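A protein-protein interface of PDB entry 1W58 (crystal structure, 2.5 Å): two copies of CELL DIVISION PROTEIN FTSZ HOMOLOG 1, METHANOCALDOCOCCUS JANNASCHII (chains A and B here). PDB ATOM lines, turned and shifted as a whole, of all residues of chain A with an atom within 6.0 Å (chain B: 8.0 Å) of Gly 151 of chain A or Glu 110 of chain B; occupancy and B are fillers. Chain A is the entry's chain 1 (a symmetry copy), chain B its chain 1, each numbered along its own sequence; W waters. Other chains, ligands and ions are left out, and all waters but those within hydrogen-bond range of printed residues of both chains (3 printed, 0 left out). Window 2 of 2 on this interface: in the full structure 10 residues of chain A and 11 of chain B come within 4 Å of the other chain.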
ATOM      1  N   GLN A 120       3.909  -7.546 -14.570  1.00  0.00           N
ATOM      2  CA  GLN A 120       4.486  -7.953 -15.850  1.00  0.00           C
ATOM      3  C   GLN A 120       3.775  -9.030 -16.662  1.00  0.00           C
ATOM      4  O   GLN A 120       3.620  -8.884 -17.874  1.00  0.00           O
ATOM      5  CB  GLN A 120       5.941  -8.393 -15.650  1.00  0.00           C
ATOM      6  CG  GLN A 120       6.622  -8.860 -16.924  1.00  0.00           C
ATOM      7  CD  GLN A 120       6.755  -7.742 -17.950  1.00  0.00           C
ATOM      8  OE1 GLN A 120       7.384  -6.719 -17.683  1.00  0.00           O
ATOM      9  NE2 GLN A 120       6.160  -7.932 -19.130  1.00  0.00           N
ATOM     10  N   SER A 122       0.564 -10.032 -16.439  1.00  0.00           N
ATOM     11  CA  SER A 122      -0.885  -9.897 -16.398  1.00  0.00           C
ATOM     12  C   SER A 122      -1.526  -9.596 -17.736  1.00  0.00           C
ATOM     13  O   SER A 122      -1.047  -8.742 -18.476  1.00  0.00           O
ATOM     14  CB  SER A 122      -1.276  -8.777 -15.434  1.00  0.00           C
ATOM     15  OG  SER A 122      -0.630  -8.929 -14.185  1.00  0.00           O
ATOM     16  N   ASP A 123      -2.632 -10.287 -18.014  1.00  0.00           N
ATOM     17  CA  ASP A 123      -3.408 -10.087 -19.233  1.00  0.00           C
ATOM     18  C   ASP A 123      -4.287  -8.878 -18.988  1.00  0.00           C
ATOM     19  O   ASP A 123      -4.633  -8.155 -19.912  1.00  0.00           O
ATOM     20  CB  ASP A 123      -4.338 -11.274 -19.514  1.00  0.00           C
ATOM     21  CG  ASP A 123      -3.606 -12.523 -20.016  1.00  0.00           C
ATOM     22  OD1 ASP A 123      -3.583 -13.534 -19.278  1.00  0.00           O
ATOM     23  OD2 ASP A 123      -3.078 -12.497 -21.153  1.00  0.00           O
ATOM     24  N   ILE A 146       2.250   2.222 -16.677  1.00  0.00           N
ATOM     25  CA  ILE A 146       3.166   1.081 -16.750  1.00  0.00           C
ATOM     26  C   ILE A 146       2.385  -0.121 -17.307  1.00  0.00           C
ATOM     27  O   ILE A 146       2.903  -0.909 -18.093  1.00  0.00           O
ATOM     28  CB  ILE A 146       3.681   0.642 -15.338  1.00  0.00           C
ATOM     29  CG1 ILE A 146       4.416   1.783 -14.619  1.00  0.00           C
ATOM     30  CG2 ILE A 146       4.518  -0.593 -15.463  1.00  0.00           C
ATOM     31  CD1 ILE A 146       5.299   2.570 -15.491  1.00  0.00           C
ATOM     32  N   SER A 147       1.137  -0.263 -16.856  1.00  0.00           N
ATOM     33  CA  SER A 147       0.265  -1.361 -17.253  1.00  0.00           C
ATOM     34  C   SER A 147       0.026  -1.367 -18.768  1.00  0.00           C
ATOM     35  O   SER A 147       0.140  -2.398 -19.418  1.00  0.00           O
ATOM     36  CB  SER A 147      -1.072  -1.247 -16.500  1.00  0.00           C
ATOM     37  OG  SER A 147      -1.878  -2.399 -16.673  1.00  0.00           O
ATOM     38  N   LYS A 148      -0.310  -0.210 -19.320  1.00  0.00           N
ATOM     39  CA  LYS A 148      -0.541  -0.108 -20.746  1.00  0.00           C
ATOM     40  C   LYS A 148       0.729  -0.360 -21.530  1.00  0.00           C
ATOM     41  O   LYS A 148       0.701  -1.008 -22.566  1.00  0.00           O
ATOM     42  CB  LYS A 148      -1.123   1.259 -21.107  1.00  0.00           C
ATOM     43  CG  LYS A 148      -2.637   1.317 -20.929  1.00  0.00           C
ATOM     44  CD  LYS A 148      -3.295   2.302 -21.893  1.00  0.00           C
ATOM     45  CE  LYS A 148      -3.168   1.855 -23.365  1.00  0.00           C
ATOM     46  NZ  LYS A 148      -3.901   0.586 -23.684  1.00  0.00           N
ATOM     47  N   LYS A 149       1.849   0.128 -21.020  1.00  0.00           N
ATOM     48  CA  LYS A 149       3.122  -0.061 -21.689  1.00  0.00           C
ATOM     49  C   LYS A 149       3.407  -1.544 -21.891  1.00  0.00           C
ATOM     50  O   LYS A 149       3.932  -1.941 -22.938  1.00  0.00           O
ATOM     51  CB  LYS A 149       4.241   0.564 -20.865  1.00  0.00           C
ATOM     52  CG  LYS A 149       5.365   1.144 -21.683  1.00  0.00           C
ATOM     53  CD  LYS A 149       5.534   2.627 -21.362  1.00  0.00           C
ATOM     54  CE  LYS A 149       4.204   3.414 -21.470  1.00  0.00           C
ATOM     55  NZ  LYS A 149       4.394   4.909 -21.446  1.00  0.00           N
ATOM     56  N   ILE A 150       3.065  -2.373 -20.907  1.00  0.00           N
ATOM     57  CA  ILE A 150       3.338  -3.796 -21.058  1.00  0.00           C
ATOM     58  C   ILE A 150       2.293  -4.576 -21.854  1.00  0.00           C
ATOM     59  O   ILE A 150       2.468  -5.774 -22.102  1.00  0.00           O
ATOM     60  CB  ILE A 150       3.548  -4.507 -19.702  1.00  0.00           C
ATOM     61  CG1 ILE A 150       2.232  -4.612 -18.955  1.00  0.00           C
ATOM     62  CG2 ILE A 150       4.592  -3.772 -18.877  1.00  0.00           C
ATOM     63  CD1 ILE A 150       2.310  -5.547 -17.796  1.00  0.00           C
ATOM     64  N   GLY A 151       1.215  -3.910 -22.253  1.00  0.00           N
ATOM     65  CA  GLY A 151       0.198  -4.578 -23.045  1.00  0.00           C
ATOM     66  C   GLY A 151      -1.043  -5.160 -22.375  1.00  0.00           C
ATOM     67  O   GLY A 151      -1.851  -5.811 -23.052  1.00  0.00           O
ATOM     68  N   ALA A 152      -1.218  -4.927 -21.074  1.00  0.00           N
ATOM     69  CA  ALA A 152      -2.377  -5.457 -20.347  1.00  0.00           C
ATOM     70  C   ALA A 152      -3.600  -4.576 -20.506  1.00  0.00           C
ATOM     71  O   ALA A 152      -3.471  -3.381 -20.734  1.00  0.00           O
ATOM     72  CB  ALA A 152      -2.043  -5.597 -18.868  1.00  0.00           C
ATOM     73  N   LEU A 153      -4.786  -5.171 -20.408  1.00  0.00           N
ATOM     74  CA  LEU A 153      -6.031  -4.401 -20.502  1.00  0.00           C
ATOM     75  C   LEU A 153      -5.983  -3.689 -19.152  1.00  0.00           C
ATOM     76  O   LEU A 153      -5.856  -4.337 -18.098  1.00  0.00           O
ATOM     77  CB  LEU A 153      -7.244  -5.347 -20.559  1.00  0.00           C
ATOM     78  CG  LEU A 153      -8.605  -5.039 -21.212  1.00  0.00           C
ATOM     79  CD1 LEU A 153      -9.670  -5.682 -20.322  1.00  0.00           C
ATOM     80  CD2 LEU A 153      -8.882  -3.561 -21.442  1.00  0.00           C
ATOM     81  N   LYS A 240     -12.241  -7.613 -23.746  1.00  0.00           N
ATOM     82  CA  LYS A 240     -11.161  -6.733 -24.173  1.00  0.00           C
ATOM     83  C   LYS A 240     -11.602  -5.764 -25.252  1.00  0.00           C
ATOM     84  O   LYS A 240     -11.207  -4.599 -25.247  1.00  0.00           O
ATOM     85  CB  LYS A 240      -9.981  -7.589 -24.653  1.00  0.00           C
ATOM     86  CG  LYS A 240      -8.655  -6.883 -24.921  1.00  0.00           C
ATOM     87  CD  LYS A 240      -7.593  -7.961 -25.213  1.00  0.00           C
ATOM     88  CE  LYS A 240      -6.150  -7.477 -25.062  1.00  0.00           C
ATOM     89  NZ  LYS A 240      -5.776  -6.423 -26.048  1.00  0.00           N
ATOM     90  N   LEU B  86       8.363 -15.715 -28.369  1.00  0.00           N
ATOM     91  CA  LEU B  86       7.011 -15.528 -28.857  1.00  0.00           C
ATOM     92  C   LEU B  86       6.698 -14.096 -28.471  1.00  0.00           C
ATOM     93  O   LEU B  86       6.622 -13.775 -27.293  1.00  0.00           O
ATOM     94  CB  LEU B  86       6.040 -16.480 -28.153  1.00  0.00           C
ATOM     95  CG  LEU B  86       4.569 -16.491 -28.604  1.00  0.00           C
ATOM     96  CD1 LEU B  86       4.481 -17.052 -30.034  1.00  0.00           C
ATOM     97  CD2 LEU B  86       3.733 -17.365 -27.620  1.00  0.00           C
ATOM     98  N   ILE B  87       6.526 -13.225 -29.451  1.00  0.00           N
ATOM     99  CA  ILE B  87       6.251 -11.832 -29.135  1.00  0.00           C
ATOM    100  C   ILE B  87       4.762 -11.541 -29.224  1.00  0.00           C
ATOM    101  O   ILE B  87       4.030 -12.254 -29.899  1.00  0.00           O
ATOM    102  CB  ILE B  87       7.042 -10.867 -30.085  1.00  0.00           C
ATOM    103  CG1 ILE B  87       6.611 -11.078 -31.534  1.00  0.00           C
ATOM    104  CG2 ILE B  87       8.538 -11.115 -29.945  1.00  0.00           C
ATOM    105  CD1 ILE B  87       6.997  -9.931 -32.498  1.00  0.00           C
ATOM    106  N   GLY B  88       4.324 -10.489 -28.540  1.00  0.00           N
ATOM    107  CA  GLY B  88       2.922 -10.117 -28.540  1.00  0.00           C
ATOM    108  C   GLY B  88       1.995 -11.105 -27.851  1.00  0.00           C
ATOM    109  O   GLY B  88       0.841 -11.232 -28.246  1.00  0.00           O
ATOM    110  N   LYS B  89       2.465 -11.795 -26.819  1.00  0.00           N
ATOM    111  CA  LYS B  89       1.617 -12.766 -26.129  1.00  0.00           C
ATOM    112  C   LYS B  89       0.266 -12.262 -25.627  1.00  0.00           C
ATOM    113  O   LYS B  89      -0.706 -13.011 -25.593  1.00  0.00           O
ATOM    114  CB  LYS B  89       2.371 -13.414 -24.970  1.00  0.00           C
ATOM    115  CG  LYS B  89       3.337 -14.461 -25.471  1.00  0.00           C
ATOM    116  CD  LYS B  89       3.774 -15.421 -24.399  1.00  0.00           C
ATOM    117  CE  LYS B  89       4.637 -14.749 -23.364  1.00  0.00           C
ATOM    118  NZ  LYS B  89       5.228 -15.775 -22.449  1.00  0.00           N
ATOM    119  N   LYS B  90       0.189 -11.001 -25.237  1.00  0.00           N
ATOM    120  CA  LYS B  90      -1.059 -10.462 -24.754  1.00  0.00           C
ATOM    121  C   LYS B  90      -1.922  -9.935 -25.896  1.00  0.00           C
ATOM    122  O   LYS B  90      -3.155 -10.045 -25.859  1.00  0.00           O
ATOM    123  CB  LYS B  90      -0.774  -9.358 -23.743  1.00  0.00           C
ATOM    124  CG  LYS B  90       0.048  -9.861 -22.577  1.00  0.00           C
ATOM    125  CD  LYS B  90       0.518  -8.727 -21.706  1.00  0.00           C
ATOM    126  CE  LYS B  90       1.408  -9.231 -20.589  1.00  0.00           C
ATOM    127  NZ  LYS B  90       2.259  -8.111 -20.112  1.00  0.00           N
ATOM    128  N   LEU B  91      -1.268  -9.375 -26.912  1.00  0.00           N
ATOM    129  CA  LEU B  91      -1.956  -8.804 -28.065  1.00  0.00           C
ATOM    130  C   LEU B  91      -2.536  -9.893 -28.980  1.00  0.00           C
ATOM    131  O   LEU B  91      -3.732 -10.033 -29.108  1.00  0.00           O
ATOM    132  CB  LEU B  91      -0.981  -7.927 -28.846  1.00  0.00           C
ATOM    133  CG  LEU B  91      -1.593  -7.178 -30.009  1.00  0.00           C
ATOM    134  CD1 LEU B  91      -2.637  -6.190 -29.455  1.00  0.00           C
ATOM    135  CD2 LEU B  91      -0.502  -6.430 -30.757  1.00  0.00           C
ATOM    136  N   THR B  92      -1.669 -10.617 -29.660  1.00  0.00           N
ATOM    137  CA  THR B  92      -2.073 -11.700 -30.531  1.00  0.00           C
ATOM    138  C   THR B  92      -1.935 -12.759 -29.479  1.00  0.00           C
ATOM    139  O   THR B  92      -1.375 -12.472 -28.419  1.00  0.00           O
ATOM    140  CB  THR B  92      -1.038 -11.910 -31.640  1.00  0.00           C
ATOM    141  OG1 THR B  92       0.251 -12.111 -31.053  1.00  0.00           O
ATOM    142  CG2 THR B  92      -0.972 -10.683 -32.534  1.00  0.00           C
ATOM    143  N   ARG B  93      -2.425 -13.961 -29.682  1.00  0.00           N
ATOM    144  CA  ARG B  93      -2.223 -14.887 -28.573  1.00  0.00           C
ATOM    145  C   ARG B  93      -1.542 -16.127 -29.063  1.00  0.00           C
ATOM    146  O   ARG B  93      -2.031 -17.233 -28.868  1.00  0.00           O
ATOM    147  CB  ARG B  93      -3.552 -15.213 -27.897  1.00  0.00           C
ATOM    148  CG  ARG B  93      -4.112 -14.044 -27.091  1.00  0.00           C
ATOM    149  CD  ARG B  93      -5.450 -14.376 -26.444  1.00  0.00           C
ATOM    150  NE  ARG B  93      -6.523 -14.538 -27.432  1.00  0.00           N
ATOM    151  CZ  ARG B  93      -7.712 -15.086 -27.173  1.00  0.00           C
ATOM    152  NH1 ARG B  93      -7.991 -15.535 -25.950  1.00  0.00           N
ATOM    153  NH2 ARG B  93      -8.623 -15.186 -28.140  1.00  0.00           N
ATOM    154  N   ILE B 103       0.080  -4.581 -35.983  1.00  0.00           N
ATOM    155  CA  ILE B 103      -0.011  -5.577 -34.937  1.00  0.00           C
ATOM    156  C   ILE B 103       1.406  -6.111 -34.668  1.00  0.00           C
ATOM    157  O   ILE B 103       1.814  -6.262 -33.517  1.00  0.00           O
ATOM    158  CB  ILE B 103      -0.918  -6.742 -35.367  1.00  0.00           C
ATOM    159  CG1 ILE B 103      -2.323  -6.234 -35.667  1.00  0.00           C
ATOM    160  CG2 ILE B 103      -0.932  -7.816 -34.305  1.00  0.00           C
ATOM    161  CD1 ILE B 103      -3.160  -6.002 -34.448  1.00  0.00           C
ATOM    162  N   GLY B 104       2.151  -6.406 -35.727  1.00  0.00           N
ATOM    163  CA  GLY B 104       3.506  -6.912 -35.543  1.00  0.00           C
ATOM    164  C   GLY B 104       4.371  -5.967 -34.726  1.00  0.00           C
ATOM    165  O   GLY B 104       5.157  -6.395 -33.883  1.00  0.00           O
ATOM    166  N   GLU B 105       4.218  -4.675 -34.992  1.00  0.00           N
ATOM    167  CA  GLU B 105       4.922  -3.611 -34.278  1.00  0.00           C
ATOM    168  C   GLU B 105       4.561  -3.530 -32.766  1.00  0.00           C
ATOM    169  O   GLU B 105       5.465  -3.535 -31.909  1.00  0.00           O
ATOM    170  CB  GLU B 105       4.605  -2.287 -34.948  1.00  0.00           C
ATOM    171  CG  GLU B 105       5.405  -1.122 -34.423  1.00  0.00           C
ATOM    172  CD  GLU B 105       5.112   0.161 -35.160  1.00  0.00           C
ATOM    173  OE1 GLU B 105       5.532   1.213 -34.667  1.00  0.00           O
ATOM    174  OE2 GLU B 105       4.470   0.129 -36.233  1.00  0.00           O
ATOM    175  N   GLU B 106       3.263  -3.463 -32.433  1.00  0.00           N
ATOM    176  CA  GLU B 106       2.851  -3.407 -31.017  1.00  0.00           C
ATOM    177  C   GLU B 106       3.287  -4.687 -30.289  1.00  0.00           C
ATOM    178  O   GLU B 106       3.654  -4.646 -29.115  1.00  0.00           O
ATOM    179  CB  GLU B 106       1.323  -3.235 -30.869  1.00  0.00           C
ATOM    180  CG  GLU B 106       0.853  -2.282 -29.731  1.00  0.00           C
ATOM    181  CD  GLU B 106       1.180  -2.724 -28.263  1.00  0.00           C
ATOM    182  OE1 GLU B 106       2.365  -2.628 -27.836  1.00  0.00           O
ATOM    183  OE2 GLU B 106       0.238  -3.150 -27.532  1.00  0.00           O
ATOM    184  N   ALA B 107       3.230  -5.825 -30.974  1.00  0.00           N
ATOM    185  CA  ALA B 107       3.649  -7.074 -30.361  1.00  0.00           C
ATOM    186  C   ALA B 107       5.143  -6.994 -30.011  1.00  0.00           C
ATOM    187  O   ALA B 107       5.536  -7.426 -28.951  1.00  0.00           O
ATOM    188  CB  ALA B 107       3.388  -8.256 -31.315  1.00  0.00           C
ATOM    189  N   ALA B 108       5.965  -6.432 -30.904  1.00  0.00           N
ATOM    190  CA  ALA B 108       7.400  -6.333 -30.651  1.00  0.00           C
ATOM    191  C   ALA B 108       7.683  -5.350 -29.541  1.00  0.00           C
ATOM    192  O   ALA B 108       8.523  -5.611 -28.697  1.00  0.00           O
ATOM    193  CB  ALA B 108       8.156  -5.914 -31.909  1.00  0.00           C
ATOM    194  N   LYS B 109       6.997  -4.211 -29.554  1.00  0.00           N
ATOM    195  CA  LYS B 109       7.182  -3.215 -28.505  1.00  0.00           C
ATOM    196  C   LYS B 109       6.789  -3.843 -27.176  1.00  0.00           C
ATOM    197  O   LYS B 109       7.458  -3.665 -26.161  1.00  0.00           O
ATOM    198  CB  LYS B 109       6.317  -1.997 -28.765  1.00  0.00           C
ATOM    199  CG  LYS B 109       6.836  -1.023 -29.837  1.00  0.00           C
ATOM    200  CD  LYS B 109       5.864   0.169 -29.877  1.00  0.00           C
ATOM    201  CE  LYS B 109       6.383   1.345 -30.666  1.00  0.00           C
ATOM    202  NZ  LYS B 109       6.392   1.081 -32.113  1.00  0.00           N
ATOM    203  N   GLU B 110       5.715  -4.616 -27.189  1.00  0.00           N
ATOM    204  CA  GLU B 110       5.252  -5.277 -25.988  1.00  0.00           C
ATOM    205  C   GLU B 110       6.300  -6.236 -25.399  1.00  0.00           C
ATOM    206  O   GLU B 110       6.379  -6.394 -24.181  1.00  0.00           O
ATOM    207  CB  GLU B 110       3.955  -5.993 -26.328  1.00  0.00           C
ATOM    208  CG  GLU B 110       3.305  -6.826 -25.252  1.00  0.00           C
ATOM    209  CD  GLU B 110       1.944  -7.383 -25.725  1.00  0.00           C
ATOM    210  OE1 GLU B 110       1.014  -6.570 -26.020  1.00  0.00           O
ATOM    211  OE2 GLU B 110       1.813  -8.628 -25.811  1.00  0.00           O
ATOM    212  N   SER B 111       7.119  -6.870 -26.243  1.00  0.00           N
ATOM    213  CA  SER B 111       8.135  -7.804 -25.745  1.00  0.00           C
ATOM    214  C   SER B 111       9.580  -7.259 -25.868  1.00  0.00           C
ATOM    215  O   SER B 111      10.530  -8.039 -25.895  1.00  0.00           O
ATOM    216  CB  SER B 111       8.044  -9.135 -26.503  1.00  0.00           C
ATOM    217  OG  SER B 111       6.713  -9.629 -26.592  1.00  0.00           O
ATOM    218  N   ALA B 112       9.736  -5.935 -25.929  1.00  0.00           N
ATOM    219  CA  ALA B 112      11.039  -5.302 -26.079  1.00  0.00           C
ATOM    220  C   ALA B 112      12.086  -5.771 -25.087  1.00  0.00           C
ATOM    221  O   ALA B 112      13.237  -5.962 -25.442  1.00  0.00           O
ATOM    222  CB  ALA B 112      10.896  -3.806 -25.984  1.00  0.00           C
ATOM    223  N   GLU B 113      11.689  -5.957 -23.841  1.00  0.00           N
ATOM    224  CA  GLU B 113      12.611  -6.410 -22.808  1.00  0.00           C
ATOM    225  C   GLU B 113      13.242  -7.758 -23.157  1.00  0.00           C
ATOM    226  O   GLU B 113      14.454  -7.926 -23.034  1.00  0.00           O
ATOM    227  CB  GLU B 113      11.876  -6.547 -21.478  1.00  0.00           C
ATOM    228  CG  GLU B 113      12.756  -6.392 -20.266  1.00  0.00           C
ATOM    229  CD  GLU B 113      12.762  -4.963 -19.761  1.00  0.00           C
ATOM    230  OE1 GLU B 113      13.657  -4.632 -18.950  1.00  0.00           O
ATOM    231  OE2 GLU B 113      11.865  -4.181 -20.170  1.00  0.00           O
ATOM    232  N   GLU B 114      12.421  -8.725 -23.563  1.00  0.00           N
ATOM    233  CA  GLU B 114      12.941 -10.045 -23.934  1.00  0.00           C
ATOM    234  C   GLU B 114      13.779  -9.981 -25.192  1.00  0.00           C
ATOM    235  O   GLU B 114      14.749 -10.723 -25.318  1.00  0.00           O
ATOM    236  CB  GLU B 114      11.827 -11.048 -24.222  1.00  0.00           C
ATOM    237  CG  GLU B 114      11.133 -11.673 -23.043  1.00  0.00           C
ATOM    238  CD  GLU B 114      10.065 -12.649 -23.514  1.00  0.00           C
ATOM    239  OE1 GLU B 114      10.406 -13.812 -23.845  1.00  0.00           O
ATOM    240  OE2 GLU B 114       8.887 -12.233 -23.585  1.00  0.00           O
ATOM    241  N   ILE B 115      13.394  -9.126 -26.137  1.00  0.00           N
ATOM    242  CA  ILE B 115      14.152  -9.033 -27.378  1.00  0.00           C
ATOM    243  C   ILE B 115      15.550  -8.513 -27.020  1.00  0.00           C
ATOM    244  O   ILE B 115      16.557  -9.098 -27.412  1.00  0.00           O
ATOM    245  CB  ILE B 115      13.446  -8.091 -28.417  1.00  0.00           C
ATOM    246  CG1 ILE B 115      12.141  -8.730 -28.924  1.00  0.00           C
ATOM    247  CG2 ILE B 115      14.345  -7.817 -29.593  1.00  0.00           C
ATOM    248  CD1 ILE B 115      11.344  -7.841 -29.905  1.00  0.00           C
ATOM    249  N   VAL B 142      11.599  -2.500 -34.919  1.00  0.00           N
ATOM    250  CA  VAL B 142      11.623  -2.459 -33.466  1.00  0.00           C
ATOM    251  C   VAL B 142      12.855  -3.195 -32.987  1.00  0.00           C
ATOM    252  O   VAL B 142      13.563  -2.716 -32.120  1.00  0.00           O
ATOM    253  CB  VAL B 142      10.314  -3.065 -32.889  1.00  0.00           C
ATOM    254  CG1 VAL B 142      10.320  -3.060 -31.375  1.00  0.00           C
ATOM    255  CG2 VAL B 142       9.135  -2.249 -33.401  1.00  0.00           C
HETATM  256  O   HOH W   1       4.358  -0.864 -25.596  1.00  0.00           O
HETATM  257  O   HOH W   2       5.143  -7.213 -21.779  1.00  0.00           O
HETATM  258  O   HOH W   3      -4.426 -11.362 -23.706  1.00  0.00           O
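No position is printed for both chains.
Among the printed residues, pairs that only touch across the chains: Ser 122 of chain A with Lys 90 of chain B (3.3 Å), Ile 150 of chain A with Glu 110 of chain B (3.4 Å), Gly 151 of chain A with Lys 90 of chain B (3.8 Å) and Gly 151 of chain A with Glu 110 of chain B (3.7 Å).
Hydrophobic or aromatic side chains of chain A that line the printed part of chain B: Ile 150.
Printed residues of chain B that touch a printed residue of chain A: Lys 90 and Glu 110.
Among the printed residues, no Asp or Glu carboxylate lies within 4 Å of a Lys or Arg side-chain nitrogen of the other chain.
Printed residues of chain B within 4 Å of Gly 151 of chain A: Lys 90 and Glu 110.
Of chain A, only Ile 150 and Gly 151 come within 4 Å of Glu 110 of chain B.
Ala 152 of chain A touches none of the printed residues of chain B.
Of the printed residues of chain B, Ile 150 of chain A touches Lys 90 (3.1 Å) and Glu 110 (3.4 Å).
Printed residues of chain B within 4 Å of Gln 120 of chain A: Lys 90.
Of the printed residues of chain B, Ser 122 of chain A touches Lys 90.
Printed residues of chain A within 4 Å of Lys 90 of chain B: Gln 120, Ser 122, Ile 150 and Gly 151.
The nearest residue of chain B that does not touch Gly 151 of chain A is Glu 106 of chain B (4.7 Å).
The nearest residue of chain A that does not touch Glu 110 of chain B is Lys 149 of chain A (4.7 Å).
Water W2 lies within hydrogen-bond range of the backbone carbonyl oxygen (O) of Glu 110 of chain B (2.8 Å), the side-chain amide nitrogen (NE2) of Gln 120 of chain A (2.9 Å), the backbone carbonyl oxygen (O) of Ile 150 of chain A (3.1 Å) and the side-chain amino group (NZ) of Lys 90 of chain B (3.5 Å).
Water W3 bridges the backbone carbonyl oxygen of Lys 90 of chain B and the side-chain carboxylate of Asp 123 of chain A.
Water W1 bridges O of Lys 149 of chain A (2.9 Å) and OE1 of Glu 106 of chain B (3.5 Å).
NZ of Lys 90 of chain B lies within hydrogen-bond range of O of Gln 120 of chain A, 2.7 Å away.
NZ of Lys 90 of chain B sits at hydrogen-bond distance from O of Ile 150 of chain A (3.1 Å).
The side-chain carboxylate of Glu 110 of chain B lies within hydrogen-bond range of the backbone NH of Lys 89 of chain B, at 3.4 Å.
N of Lys 90 of chain B sits at hydrogen-bond distance from OE2 of Glu 110 of chain B.
OE2 of Glu 110 of chain B lies within hydrogen-bond range of N of Leu 91 of chain B (3.4 Å).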
